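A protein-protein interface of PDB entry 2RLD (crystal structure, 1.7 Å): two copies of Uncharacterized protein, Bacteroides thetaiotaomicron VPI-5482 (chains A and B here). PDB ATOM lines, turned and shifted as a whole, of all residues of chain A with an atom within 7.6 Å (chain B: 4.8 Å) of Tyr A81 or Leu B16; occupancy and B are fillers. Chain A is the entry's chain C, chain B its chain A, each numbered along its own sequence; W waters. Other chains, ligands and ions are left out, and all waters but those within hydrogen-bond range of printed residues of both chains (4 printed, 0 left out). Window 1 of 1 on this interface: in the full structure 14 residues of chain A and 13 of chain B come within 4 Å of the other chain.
Of the 14 printed residues of chain B, 8 touch a printed residue of chain A. Printed residues of chain B that touch a printed residue of chain A: Leu B16, Glu B17, Ala B19, Val B20, Thr B47, Gly B50, Ala B51 and Arg B54. Among the printed residues, Asp or Glu carboxylates within 4 Å of a Lys or Arg side-chain nitrogen of the other chain: Arg A88 with Glu B17 (3.0 Å).
Glu A80 touches Arg B54. Tyr A81 touches Gly B50. CZ of Tyr A81 touches N of Ala B51 (3.4 Å). Arg B54 touches Tyr A81 (NH1 to CA, 3.5 Å). Trp A82 touches Thr B47 (CH2 to O, 3.5 Å). Trp A82 touches Ala B51. OE2 of Glu A84 touches CD1 of Leu B16 (3.7 Å). Leu A85 touches Thr B47. NH1 of Arg A88 touches CD1 of Leu B16, 3.6 Å away. CB of Arg A88 touches CG2 of Val B20, 3.7 Å away.
No position is printed for both chains.
Water W2 lies within hydrogen-bond range of the side-chain carboxylate of Glu A84, the guanidinium group of Arg B54 and the backbone carbonyl oxygen of Glu A80. Water W4 lies within hydrogen-bond range of O of Ser B15 (2.8 Å), N of Gly B50 (3.0 Å) and OH of Tyr A81 (3.5 Å). Water W1 bridges OG1 of Thr B47 (2.9 Å) and NE2 of Gln A41 (3.0 Å). Water W3 bridges OG of Ser B48 (3.0 Å) and NE2 of Gln A41 (3.2 Å).
OE2 of Glu B17 lies within salt-bridge range of NH1 of Arg A88, at 3.0 Å. O of Thr B47 lies within hydrogen-bond range of OH of Tyr A81 (2.6 Å). The guanidinium group (NH2) of Arg B54 sits at hydrogen-bond distance from the backbone carbonyl oxygen (O) of Asn A77 (3.1 Å).
The side-chain carboxylate of Glu A78 sits at hydrogen-bond distance from the indole nitrogen of Trp A82, 2.8 Å away. OE2 of Glu A80 lies within hydrogen-bond range of OG of Ser A104. OG1 of Thr A89 lies within hydrogen-bond range of O of Leu A85.
Printed residues of chain B within 4 Å of Asn A77: Arg B54. Of the printed residues of chain B, Glu A84 touches Leu B16 (3.7 Å). Of the printed residues of chain B, Leu A85 touches Ala B19, Val B20 and Thr B47. Ser B15 touches none of the printed residues of chain A. Leu B16 touches three residues of chain A. Printed residues of chain A within 4 Å of Ala B19: Tyr A81 (3.3 Å) and Leu A85 (3.8 Å). Printed residues of chain A within 4 Å of Arg B54: Asn A77 (3.1 Å), Glu A80 (3.7 Å) and Tyr A81 (3.5 Å). The nearest residue of chain B that does not touch Tyr A81 is Ser B15 (4.2 Å).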
ATOM      1  N   MET A  38     -18.582  14.117  38.620  1.00  0.00           N
ATOM      2  CA  MET A  38     -18.575  14.032  37.183  1.00  0.00           C
ATOM      3  C   MET A  38     -18.487  15.421  36.541  1.00  0.00           C
ATOM      4  O   MET A  38     -17.795  15.624  35.532  1.00  0.00           O
ATOM      5  CB  MET A  38     -19.773  13.203  36.695  1.00  0.00           C
ATOM      6  CG  MET A  38     -19.795  11.846  37.324  1.00  0.00           C
ATOM      7  SD  MET A  38     -21.267  10.795  36.620  1.00  0.00           S
ATOM      8  CE  MET A  38     -22.769  11.655  37.665  1.00  0.00           C
ATOM      9  N   GLN A  41     -14.958  16.658  36.285  1.00  0.00           N
ATOM     10  CA  GLN A  41     -14.232  15.919  35.253  1.00  0.00           C
ATOM     11  C   GLN A  41     -14.561  16.478  33.879  1.00  0.00           C
ATOM     12  O   GLN A  41     -13.670  16.750  33.078  1.00  0.00           O
ATOM     13  CB  GLN A  41     -14.553  14.446  35.287  1.00  0.00           C
ATOM     14  CG  GLN A  41     -14.118  13.729  36.538  1.00  0.00           C
ATOM     15  CD  GLN A  41     -12.714  13.240  36.469  1.00  0.00           C
ATOM     16  OE1 GLN A  41     -11.843  13.912  35.913  1.00  0.00           O
ATOM     17  NE2 GLN A  41     -12.469  12.058  37.037  1.00  0.00           N
ATOM     18  N   ILE A  42     -15.844  16.721  33.615  1.00  0.00           N
ATOM     19  CA  ILE A  42     -16.253  17.166  32.286  1.00  0.00           C
ATOM     20  C   ILE A  42     -15.978  18.645  32.062  1.00  0.00           C
ATOM     21  O   ILE A  42     -15.761  19.065  30.918  1.00  0.00           O
ATOM     22  CB  ILE A  42     -17.743  16.810  31.988  1.00  0.00           C
ATOM     23  CG1 ILE A  42     -17.978  16.824  30.475  1.00  0.00           C
ATOM     24  CG2 ILE A  42     -18.716  17.709  32.739  1.00  0.00           C
ATOM     25  CD1 ILE A  42     -19.404  16.515  30.051  1.00  0.00           C
ATOM     26  N   SER A  45     -12.318  18.265  30.849  1.00  0.00           N
ATOM     27  CA  SER A  45     -12.134  17.686  29.535  1.00  0.00           C
ATOM     28  C   SER A  45     -12.773  18.566  28.468  1.00  0.00           C
ATOM     29  O   SER A  45     -12.152  18.835  27.450  1.00  0.00           O
ATOM     30  CB  SER A  45     -12.627  16.225  29.469  1.00  0.00           C
ATOM     31  OG  SER A  45     -14.035  16.081  29.579  1.00  0.00           O
ATOM     32  N   GLU A  75      -9.522  14.696  24.396  1.00  0.00           N
ATOM     33  CA  GLU A  75     -10.366  15.450  25.338  1.00  0.00           C
ATOM     34  C   GLU A  75     -11.836  15.449  24.878  1.00  0.00           C
ATOM     35  O   GLU A  75     -12.758  15.305  25.688  1.00  0.00           O
ATOM     36  CB  GLU A  75      -9.816  16.867  25.512  1.00  0.00           C
ATOM     37  CG  GLU A  75      -8.425  16.957  26.160  1.00  0.00           C
ATOM     38  CD  GLU A  75      -8.370  16.555  27.636  1.00  0.00           C
ATOM     39  OE1 GLU A  75      -9.370  16.073  28.207  1.00  0.00           O
ATOM     40  OE2 GLU A  75      -7.293  16.764  28.240  1.00  0.00           O
ATOM     41  N   ALA A  76     -12.061  15.562  23.577  1.00  0.00           N
ATOM     42  CA  ALA A  76     -13.414  15.437  23.001  1.00  0.00           C
ATOM     43  C   ALA A  76     -14.015  14.061  23.309  1.00  0.00           C
ATOM     44  O   ALA A  76     -15.181  13.959  23.718  1.00  0.00           O
ATOM     45  CB  ALA A  76     -13.368  15.679  21.496  1.00  0.00           C
ATOM     46  N   ASN A  77     -13.211  13.016  23.155  1.00  0.00           N
ATOM     47  CA  ASN A  77     -13.687  11.680  23.442  1.00  0.00           C
ATOM     48  C   ASN A  77     -13.963  11.454  24.906  1.00  0.00           C
ATOM     49  O   ASN A  77     -14.991  10.851  25.248  1.00  0.00           O
ATOM     50  CB  ASN A  77     -12.738  10.637  22.900  1.00  0.00           C
ATOM     51  CG  ASN A  77     -13.024  10.334  21.470  1.00  0.00           C
ATOM     52  OD1 ASN A  77     -13.950   9.572  21.177  1.00  0.00           O
ATOM     53  ND2 ASN A  77     -12.273  10.947  20.563  1.00  0.00           N
ATOM     54  N   GLU A  78     -13.107  11.977  25.779  1.00  0.00           N
ATOM     55  CA  GLU A  78     -13.394  11.851  27.222  1.00  0.00           C
ATOM     56  C   GLU A  78     -14.686  12.585  27.587  1.00  0.00           C
ATOM     57  O   GLU A  78     -15.509  12.082  28.368  1.00  0.00           O
ATOM     58  CB  GLU A  78     -12.231  12.366  28.062  1.00  0.00           C
ATOM     59  CG  GLU A  78     -12.453  12.028  29.528  1.00  0.00           C
ATOM     60  CD  GLU A  78     -11.451  12.623  30.478  1.00  0.00           C
ATOM     61  OE1 GLU A  78     -10.308  12.910  30.055  1.00  0.00           O
ATOM     62  OE2 GLU A  78     -11.826  12.793  31.662  1.00  0.00           O
ATOM     63  N   THR A  79     -14.870  13.753  27.005  1.00  0.00           N
ATOM     64  CA  THR A  79     -16.066  14.567  27.260  1.00  0.00           C
ATOM     65  C   THR A  79     -17.309  13.763  26.851  1.00  0.00           C
ATOM     66  O   THR A  79     -18.311  13.767  27.551  1.00  0.00           O
ATOM     67  CB  THR A  79     -15.997  15.911  26.480  1.00  0.00           C
ATOM     68  OG1 THR A  79     -14.848  16.668  26.905  1.00  0.00           O
ATOM     69  CG2 THR A  79     -17.263  16.746  26.689  1.00  0.00           C
ATOM     70  N   GLU A  80     -17.230  13.098  25.707  1.00  0.00           N
ATOM     71  CA  GLU A  80     -18.339  12.255  25.204  1.00  0.00           C
ATOM     72  C   GLU A  80     -18.650  11.107  26.172  1.00  0.00           C
ATOM     73  O   GLU A  80     -19.802  10.747  26.377  1.00  0.00           O
ATOM     74  CB  GLU A  80     -18.017  11.814  23.770  1.00  0.00           C
ATOM     75  CG  GLU A  80     -18.207  13.019  22.814  1.00  0.00           C
ATOM     76  CD  GLU A  80     -17.218  13.107  21.662  1.00  0.00           C
ATOM     77  OE1 GLU A  80     -16.541  12.100  21.366  1.00  0.00           O
ATOM     78  OE2 GLU A  80     -17.117  14.213  21.070  1.00  0.00           O
ATOM     79  N   TYR A  81     -17.614  10.552  26.782  1.00  0.00           N
ATOM     80  CA  TYR A  81     -17.782   9.538  27.828  1.00  0.00           C
ATOM     81  C   TYR A  81     -18.580  10.115  28.981  1.00  0.00           C
ATOM     82  O   TYR A  81     -19.581   9.534  29.416  1.00  0.00           O
ATOM     83  CB  TYR A  81     -16.404   9.071  28.336  1.00  0.00           C
ATOM     84  CG  TYR A  81     -16.443   8.207  29.611  1.00  0.00           C
ATOM     85  CD1 TYR A  81     -16.730   6.860  29.564  1.00  0.00           C
ATOM     86  CD2 TYR A  81     -16.164   8.770  30.838  1.00  0.00           C
ATOM     87  CE1 TYR A  81     -16.755   6.084  30.741  1.00  0.00           C
ATOM     88  CE2 TYR A  81     -16.208   8.023  32.023  1.00  0.00           C
ATOM     89  CZ  TYR A  81     -16.513   6.688  31.964  1.00  0.00           C
ATOM     90  OH  TYR A  81     -16.496   5.959  33.135  1.00  0.00           O
ATOM     91  N   TRP A  82     -18.148  11.268  29.482  1.00  0.00           N
ATOM     92  CA  TRP A  82     -18.856  11.862  30.636  1.00  0.00           C
ATOM     93  C   TRP A  82     -20.297  12.207  30.264  1.00  0.00           C
ATOM     94  O   TRP A  82     -21.212  11.975  31.063  1.00  0.00           O
ATOM     95  CB  TRP A  82     -18.123  13.099  31.222  1.00  0.00           C
ATOM     96  CG  TRP A  82     -16.798  12.745  31.850  1.00  0.00           C
ATOM     97  CD1 TRP A  82     -15.541  13.089  31.403  1.00  0.00           C
ATOM     98  CD2 TRP A  82     -16.604  11.940  33.015  1.00  0.00           C
ATOM     99  NE1 TRP A  82     -14.582  12.543  32.244  1.00  0.00           N
ATOM    100  CE2 TRP A  82     -15.209  11.826  33.225  1.00  0.00           C
ATOM    101  CE3 TRP A  82     -17.486  11.290  33.903  1.00  0.00           C
ATOM    102  CZ2 TRP A  82     -14.677  11.102  34.279  1.00  0.00           C
ATOM    103  CZ3 TRP A  82     -16.950  10.599  34.968  1.00  0.00           C
ATOM    104  CH2 TRP A  82     -15.552  10.497  35.139  1.00  0.00           C
ATOM    105  N   LEU A  83     -20.521  12.689  29.041  1.00  0.00           N
ATOM    106  CA  LEU A  83     -21.893  13.020  28.634  1.00  0.00           C
ATOM    107  C   LEU A  83     -22.772  11.763  28.630  1.00  0.00           C
ATOM    108  O   LEU A  83     -23.936  11.772  29.033  1.00  0.00           O
ATOM    109  CB  LEU A  83     -21.894  13.671  27.259  1.00  0.00           C
ATOM    110  CG  LEU A  83     -21.375  15.106  27.195  1.00  0.00           C
ATOM    111  CD1 LEU A  83     -21.227  15.553  25.733  1.00  0.00           C
ATOM    112  CD2 LEU A  83     -22.283  16.097  28.005  1.00  0.00           C
ATOM    113  N   GLU A  84     -22.226  10.674  28.128  1.00  0.00           N
ATOM    114  CA  GLU A  84     -22.971   9.428  28.063  1.00  0.00           C
ATOM    115  C   GLU A  84     -23.325   8.939  29.466  1.00  0.00           C
ATOM    116  O   GLU A  84     -24.452   8.490  29.749  1.00  0.00           O
ATOM    117  CB  GLU A  84     -22.128   8.372  27.350  1.00  0.00           C
ATOM    118  CG  GLU A  84     -22.925   7.107  27.033  1.00  0.00           C
ATOM    119  CD  GLU A  84     -22.139   6.074  26.215  1.00  0.00           C
ATOM    120  OE1 GLU A  84     -21.053   6.405  25.676  1.00  0.00           O
ATOM    121  OE2 GLU A  84     -22.639   4.935  26.106  1.00  0.00           O
ATOM    122  N   LEU A  85     -22.343   9.000  30.357  1.00  0.00           N
ATOM    123  CA  LEU A  85     -22.592   8.656  31.764  1.00  0.00           C
ATOM    124  C   LEU A  85     -23.678   9.531  32.400  1.00  0.00           C
ATOM    125  O   LEU A  85     -24.566   9.026  33.096  1.00  0.00           O
ATOM    126  CB  LEU A  85     -21.283   8.744  32.559  1.00  0.00           C
ATOM    127  CG  LEU A  85     -21.280   8.181  33.967  1.00  0.00           C
ATOM    128  CD1 LEU A  85     -21.937   6.809  34.076  1.00  0.00           C
ATOM    129  CD2 LEU A  85     -19.831   8.177  34.472  1.00  0.00           C
ATOM    130  N   LEU A  86     -23.619  10.830  32.148  1.00  0.00           N
ATOM    131  CA  LEU A  86     -24.617  11.747  32.682  1.00  0.00           C
ATOM    132  C   LEU A  86     -26.050  11.470  32.192  1.00  0.00           C
ATOM    133  O   LEU A  86     -26.966  11.480  32.989  1.00  0.00           O
ATOM    134  CB  LEU A  86     -24.220  13.197  32.411  1.00  0.00           C
ATOM    135  CG  LEU A  86     -22.969  13.720  33.143  1.00  0.00           C
ATOM    136  CD1 LEU A  86     -22.446  15.008  32.498  1.00  0.00           C
ATOM    137  CD2 LEU A  86     -23.322  13.949  34.659  1.00  0.00           C
ATOM    138  N   ILE A  87     -26.246  11.174  30.902  1.00  0.00           N
ATOM    139  CA  ILE A  87     -27.602  10.798  30.435  1.00  0.00           C
ATOM    140  C   ILE A  87     -28.033   9.455  30.987  1.00  0.00           C
ATOM    141  O   ILE A  87     -29.167   9.297  31.420  1.00  0.00           O
ATOM    142  CB  ILE A  87     -27.756  10.878  28.875  1.00  0.00           C
ATOM    143  CG1 ILE A  87     -29.227  10.651  28.447  1.00  0.00           C
ATOM    144  CG2 ILE A  87     -26.855   9.887  28.162  1.00  0.00           C
ATOM    145  CD1 ILE A  87     -30.176  11.666  28.980  1.00  0.00           C
ATOM    146  N   ARG A  88     -27.124   8.475  31.023  1.00  0.00           N
ATOM    147  CA  ARG A  88     -27.492   7.150  31.557  1.00  0.00           C
ATOM    148  C   ARG A  88     -27.859   7.174  33.029  1.00  0.00           C
ATOM    149  O   ARG A  88     -28.677   6.388  33.470  1.00  0.00           O
ATOM    150  CB  ARG A  88     -26.374   6.138  31.315  1.00  0.00           C
ATOM    151  CG  ARG A  88     -26.192   5.800  29.834  1.00  0.00           C
ATOM    152  CD  ARG A  88     -27.243   4.817  29.356  1.00  0.00           C
ATOM    153  NE  ARG A  88     -27.343   3.636  30.220  1.00  0.00           N
ATOM    154  CZ  ARG A  88     -26.522   2.597  30.168  1.00  0.00           C
ATOM    155  NH1 ARG A  88     -25.500   2.578  29.324  1.00  0.00           N
ATOM    156  NH2 ARG A  88     -26.707   1.588  30.987  1.00  0.00           N
ATOM    157  N   THR A  89     -27.296   8.108  33.783  1.00  0.00           N
ATOM    158  CA  THR A  89     -27.634   8.240  35.202  1.00  0.00           C
ATOM    159  C   THR A  89     -28.619   9.396  35.504  1.00  0.00           C
ATOM    160  O   THR A  89     -28.816   9.734  36.657  1.00  0.00           O
ATOM    161  CB  THR A  89     -26.359   8.403  36.038  1.00  0.00           C
ATOM    162  OG1 THR A  89     -25.598   9.523  35.561  1.00  0.00           O
ATOM    163  CG2 THR A  89     -25.511   7.133  35.956  1.00  0.00           C
ATOM    164  N   TYR A  97     -28.501  16.156  26.466  1.00  0.00           N
ATOM    165  CA  TYR A  97     -27.499  15.218  25.960  1.00  0.00           C
ATOM    166  C   TYR A  97     -27.287  15.405  24.460  1.00  0.00           C
ATOM    167  O   TYR A  97     -26.152  15.632  24.000  1.00  0.00           O
ATOM    168  CB  TYR A  97     -27.918  13.771  26.252  1.00  0.00           C
ATOM    169  CG  TYR A  97     -26.978  12.780  25.599  1.00  0.00           C
ATOM    170  CD1 TYR A  97     -25.692  12.591  26.093  1.00  0.00           C
ATOM    171  CD2 TYR A  97     -27.366  12.047  24.488  1.00  0.00           C
ATOM    172  CE1 TYR A  97     -24.810  11.706  25.490  1.00  0.00           C
ATOM    173  CE2 TYR A  97     -26.483  11.138  23.875  1.00  0.00           C
ATOM    174  CZ  TYR A  97     -25.203  10.986  24.384  1.00  0.00           C
ATOM    175  OH  TYR A  97     -24.307  10.098  23.805  1.00  0.00           O
ATOM    176  N   ASN A 101     -23.899  16.799  22.955  1.00  0.00           N
ATOM    177  CA  ASN A 101     -23.123  15.729  22.335  1.00  0.00           C
ATOM    178  C   ASN A 101     -22.949  15.919  20.827  1.00  0.00           C
ATOM    179  O   ASN A 101     -21.909  15.578  20.277  1.00  0.00           O
ATOM    180  CB  ASN A 101     -23.744  14.361  22.626  1.00  0.00           C
ATOM    181  CG  ASN A 101     -22.848  13.215  22.179  1.00  0.00           C
ATOM    182  OD1 ASN A 101     -21.779  13.000  22.743  1.00  0.00           O
ATOM    183  ND2 ASN A 101     -23.279  12.484  21.164  1.00  0.00           N
ATOM    184  N   SER A 104     -20.175  18.268  20.404  1.00  0.00           N
ATOM    185  CA  SER A 104     -18.922  17.552  20.696  1.00  0.00           C
ATOM    186  C   SER A 104     -18.481  16.739  19.502  1.00  0.00           C
ATOM    187  O   SER A 104     -17.329  16.816  19.057  1.00  0.00           O
ATOM    188  CB  SER A 104     -19.069  16.663  21.934  1.00  0.00           C
ATOM    189  OG  SER A 104     -17.805  16.480  22.574  1.00  0.00           O
ATOM    190  N   LYS B  12     -13.882  -1.150  26.830  1.00  0.00           N
ATOM    191  CA  LYS B  12     -14.491   0.158  26.684  1.00  0.00           C
ATOM    192  C   LYS B  12     -16.008   0.119  27.049  1.00  0.00           C
ATOM    193  O   LYS B  12     -16.509   0.939  27.836  1.00  0.00           O
ATOM    194  CB  LYS B  12     -14.260   0.658  25.246  1.00  0.00           C
ATOM    195  CG  LYS B  12     -15.003   1.945  24.895  1.00  0.00           C
ATOM    196  CD  LYS B  12     -14.675   2.425  23.484  1.00  0.00           C
ATOM    197  CE  LYS B  12     -15.358   3.731  23.162  1.00  0.00           C
ATOM    198  NZ  LYS B  12     -15.119   4.189  21.747  1.00  0.00           N
ATOM    199  N   ASP B  13     -16.723  -0.844  26.491  1.00  0.00           N
ATOM    200  CA  ASP B  13     -18.162  -0.991  26.702  1.00  0.00           C
ATOM    201  C   ASP B  13     -18.448  -1.317  28.162  1.00  0.00           C
ATOM    202  O   ASP B  13     -19.303  -0.716  28.797  1.00  0.00           O
ATOM    203  CB  ASP B  13     -18.696  -2.107  25.779  1.00  0.00           C
ATOM    204  CG  ASP B  13     -20.195  -2.393  25.962  1.00  0.00           C
ATOM    205  OD1 ASP B  13     -21.020  -1.487  25.746  1.00  0.00           O
ATOM    206  OD2 ASP B  13     -20.558  -3.545  26.291  1.00  0.00           O
ATOM    207  N   LYS B  14     -17.727  -2.296  28.684  1.00  0.00           N
ATOM    208  CA  LYS B  14     -17.940  -2.761  30.052  1.00  0.00           C
ATOM    209  C   LYS B  14     -17.646  -1.664  31.088  1.00  0.00           C
ATOM    210  O   LYS B  14     -18.307  -1.595  32.127  1.00  0.00           O
ATOM    211  CB  LYS B  14     -17.061  -3.983  30.338  1.00  0.00           C
ATOM    212  CG  LYS B  14     -17.399  -5.251  29.525  1.00  0.00           C
ATOM    213  CD  LYS B  14     -18.671  -5.881  29.971  1.00  0.00           C
ATOM    214  CE  LYS B  14     -18.800  -7.326  29.459  1.00  0.00           C
ATOM    215  NZ  LYS B  14     -20.216  -7.581  29.075  1.00  0.00           N
ATOM    216  N   SER B  15     -16.635  -0.840  30.823  1.00  0.00           N
ATOM    217  CA  SER B  15     -16.264   0.227  31.770  1.00  0.00           C
ATOM    218  C   SER B  15     -17.307   1.336  31.851  1.00  0.00           C
ATOM    219  O   SER B  15     -17.517   1.923  32.914  1.00  0.00           O
ATOM    220  CB  SER B  15     -14.872   0.766  31.506  1.00  0.00           C
ATOM    221  OG  SER B  15     -14.761   1.327  30.232  1.00  0.00           O
ATOM    222  N   LEU B  16     -17.955   1.636  30.731  1.00  0.00           N
ATOM    223  CA  LEU B  16     -19.082   2.564  30.749  1.00  0.00           C
ATOM    224  C   LEU B  16     -20.247   1.965  31.550  1.00  0.00           C
ATOM    225  O   LEU B  16     -20.774   2.588  32.453  1.00  0.00           O
ATOM    226  CB  LEU B  16     -19.525   2.922  29.326  1.00  0.00           C
ATOM    227  CG  LEU B  16     -20.604   4.018  29.171  1.00  0.00           C
ATOM    228  CD1 LEU B  16     -21.974   3.426  29.385  1.00  0.00           C
ATOM    229  CD2 LEU B  16     -20.399   5.255  30.055  1.00  0.00           C
ATOM    230  N   GLU B  17     -20.633   0.739  31.243  1.00  0.00           N
ATOM    231  CA  GLU B  17     -21.694   0.097  32.027  1.00  0.00           C
ATOM    232  C   GLU B  17     -21.389   0.012  33.532  1.00  0.00           C
ATOM    233  O   GLU B  17     -22.262   0.196  34.382  1.00  0.00           O
ATOM    234  CB  GLU B  17     -21.969  -1.290  31.468  1.00  0.00           C
ATOM    235  CG  GLU B  17     -22.487  -1.256  30.039  1.00  0.00           C
ATOM    236  CD  GLU B  17     -23.838  -0.570  29.894  1.00  0.00           C
ATOM    237  OE1 GLU B  17     -24.665  -0.587  30.835  1.00  0.00           O
ATOM    238  OE2 GLU B  17     -24.067   0.011  28.825  1.00  0.00           O
ATOM    239  N   PHE B  18     -20.130  -0.214  33.835  1.00  0.00           N
ATOM    240  CA  PHE B  18     -19.699  -0.311  35.215  1.00  0.00           C
ATOM    241  C   PHE B  18     -19.778   1.052  35.890  1.00  0.00           C
ATOM    242  O   PHE B  18     -20.167   1.124  37.031  1.00  0.00           O
ATOM    243  CB  PHE B  18     -18.299  -0.900  35.310  1.00  0.00           C
ATOM    244  CG  PHE B  18     -17.831  -1.091  36.710  1.00  0.00           C
ATOM    245  CD1 PHE B  18     -18.370  -2.072  37.501  1.00  0.00           C
ATOM    246  CD2 PHE B  18     -16.826  -0.279  37.237  1.00  0.00           C
ATOM    247  CE1 PHE B  18     -17.904  -2.257  38.804  1.00  0.00           C
ATOM    248  CE2 PHE B  18     -16.337  -0.484  38.546  1.00  0.00           C
ATOM    249  CZ  PHE B  18     -16.878  -1.467  39.306  1.00  0.00           C
ATOM    250  N   ALA B  19     -19.401   2.126  35.193  1.00  0.00           N
ATOM    251  CA  ALA B  19     -19.498   3.492  35.751  1.00  0.00           C
ATOM    252  C   ALA B  19     -20.950   3.810  36.100  1.00  0.00           C
ATOM    253  O   ALA B  19     -21.246   4.390  37.149  1.00  0.00           O
ATOM    254  CB  ALA B  19     -18.939   4.502  34.734  1.00  0.00           C
ATOM    255  N   VAL B  20     -21.861   3.332  35.256  1.00  0.00           N
ATOM    256  CA  VAL B  20     -23.292   3.499  35.508  1.00  0.00           C
ATOM    257  C   VAL B  20     -23.685   2.796  36.801  1.00  0.00           C
ATOM    258  O   VAL B  20     -24.388   3.402  37.665  1.00  0.00           O
ATOM    259  CB  VAL B  20     -24.158   3.020  34.300  1.00  0.00           C
ATOM    260  CG1 VAL B  20     -25.658   3.039  34.655  1.00  0.00           C
ATOM    261  CG2 VAL B  20     -23.906   3.915  33.046  1.00  0.00           C
ATOM    262  N   THR B  47     -15.950   5.633  38.376  1.00  0.00           N
ATOM    263  CA  THR B  47     -16.272   6.334  37.125  1.00  0.00           C
ATOM    264  C   THR B  47     -15.014   6.746  36.315  1.00  0.00           C
ATOM    265  O   THR B  47     -15.094   6.992  35.094  1.00  0.00           O
ATOM    266  CB  THR B  47     -17.205   7.540  37.368  1.00  0.00           C
ATOM    267  OG1 THR B  47     -16.585   8.535  38.206  1.00  0.00           O
ATOM    268  CG2 THR B  47     -18.540   7.103  38.010  1.00  0.00           C
ATOM    269  N   SER B  48     -13.872   6.806  37.002  1.00  0.00           N
ATOM    270  CA  SER B  48     -12.608   7.223  36.406  1.00  0.00           C
ATOM    271  C   SER B  48     -12.056   6.150  35.491  1.00  0.00           C
ATOM    272  O   SER B  48     -11.393   6.446  34.500  1.00  0.00           O
ATOM    273  CB  SER B  48     -11.572   7.501  37.499  1.00  0.00           C
ATOM    274  OG  SER B  48     -10.382   8.017  36.943  1.00  0.00           O
ATOM    275  N   GLY B  50     -13.372   4.096  33.233  1.00  0.00           N
ATOM    276  CA  GLY B  50     -13.787   4.199  31.831  1.00  0.00           C
ATOM    277  C   GLY B  50     -13.258   5.446  31.138  1.00  0.00           C
ATOM    278  O   GLY B  50     -12.997   5.415  29.943  1.00  0.00           O
ATOM    279  N   ALA B  51     -13.118   6.545  31.885  1.00  0.00           N
ATOM    280  CA  ALA B  51     -12.536   7.786  31.335  1.00  0.00           C
ATOM    281  C   ALA B  51     -11.097   7.531  30.876  1.00  0.00           C
ATOM    282  O   ALA B  51     -10.715   7.906  29.751  1.00  0.00           O
ATOM    283  CB  ALA B  51     -12.590   8.926  32.360  1.00  0.00           C
ATOM    284  N   ARG B  54     -11.106   5.368  27.766  1.00  0.00           N
ATOM    285  CA  ARG B  54     -11.379   6.207  26.591  1.00  0.00           C
ATOM    286  C   ARG B  54     -10.134   6.970  26.143  1.00  0.00           C
ATOM    287  O   ARG B  54      -9.826   6.998  24.946  1.00  0.00           O
ATOM    288  CB  ARG B  54     -12.512   7.193  26.843  1.00  0.00           C
ATOM    289  CG  ARG B  54     -13.842   6.564  26.937  1.00  0.00           C
ATOM    290  CD  ARG B  54     -14.322   6.058  25.586  1.00  0.00           C
ATOM    291  NE  ARG B  54     -14.769   7.100  24.658  1.00  0.00           N
ATOM    292  CZ  ARG B  54     -16.014   7.590  24.603  1.00  0.00           C
ATOM    293  NH1 ARG B  54     -16.955   7.143  25.410  1.00  0.00           N
ATOM    294  NH2 ARG B  54     -16.334   8.516  23.709  1.00  0.00           N
HETATM  295  O   HOH W   1     -14.276  10.231  38.559  1.00  0.00           O
HETATM  296  O   HOH W   2     -19.639   8.157  24.566  1.00  0.00           O
HETATM  297  O   HOH W   3      -9.754  10.668  38.090  1.00  0.00           O
HETATM  298  O   HOH W   4     -15.699   3.006  34.733  1.00  0.00           O
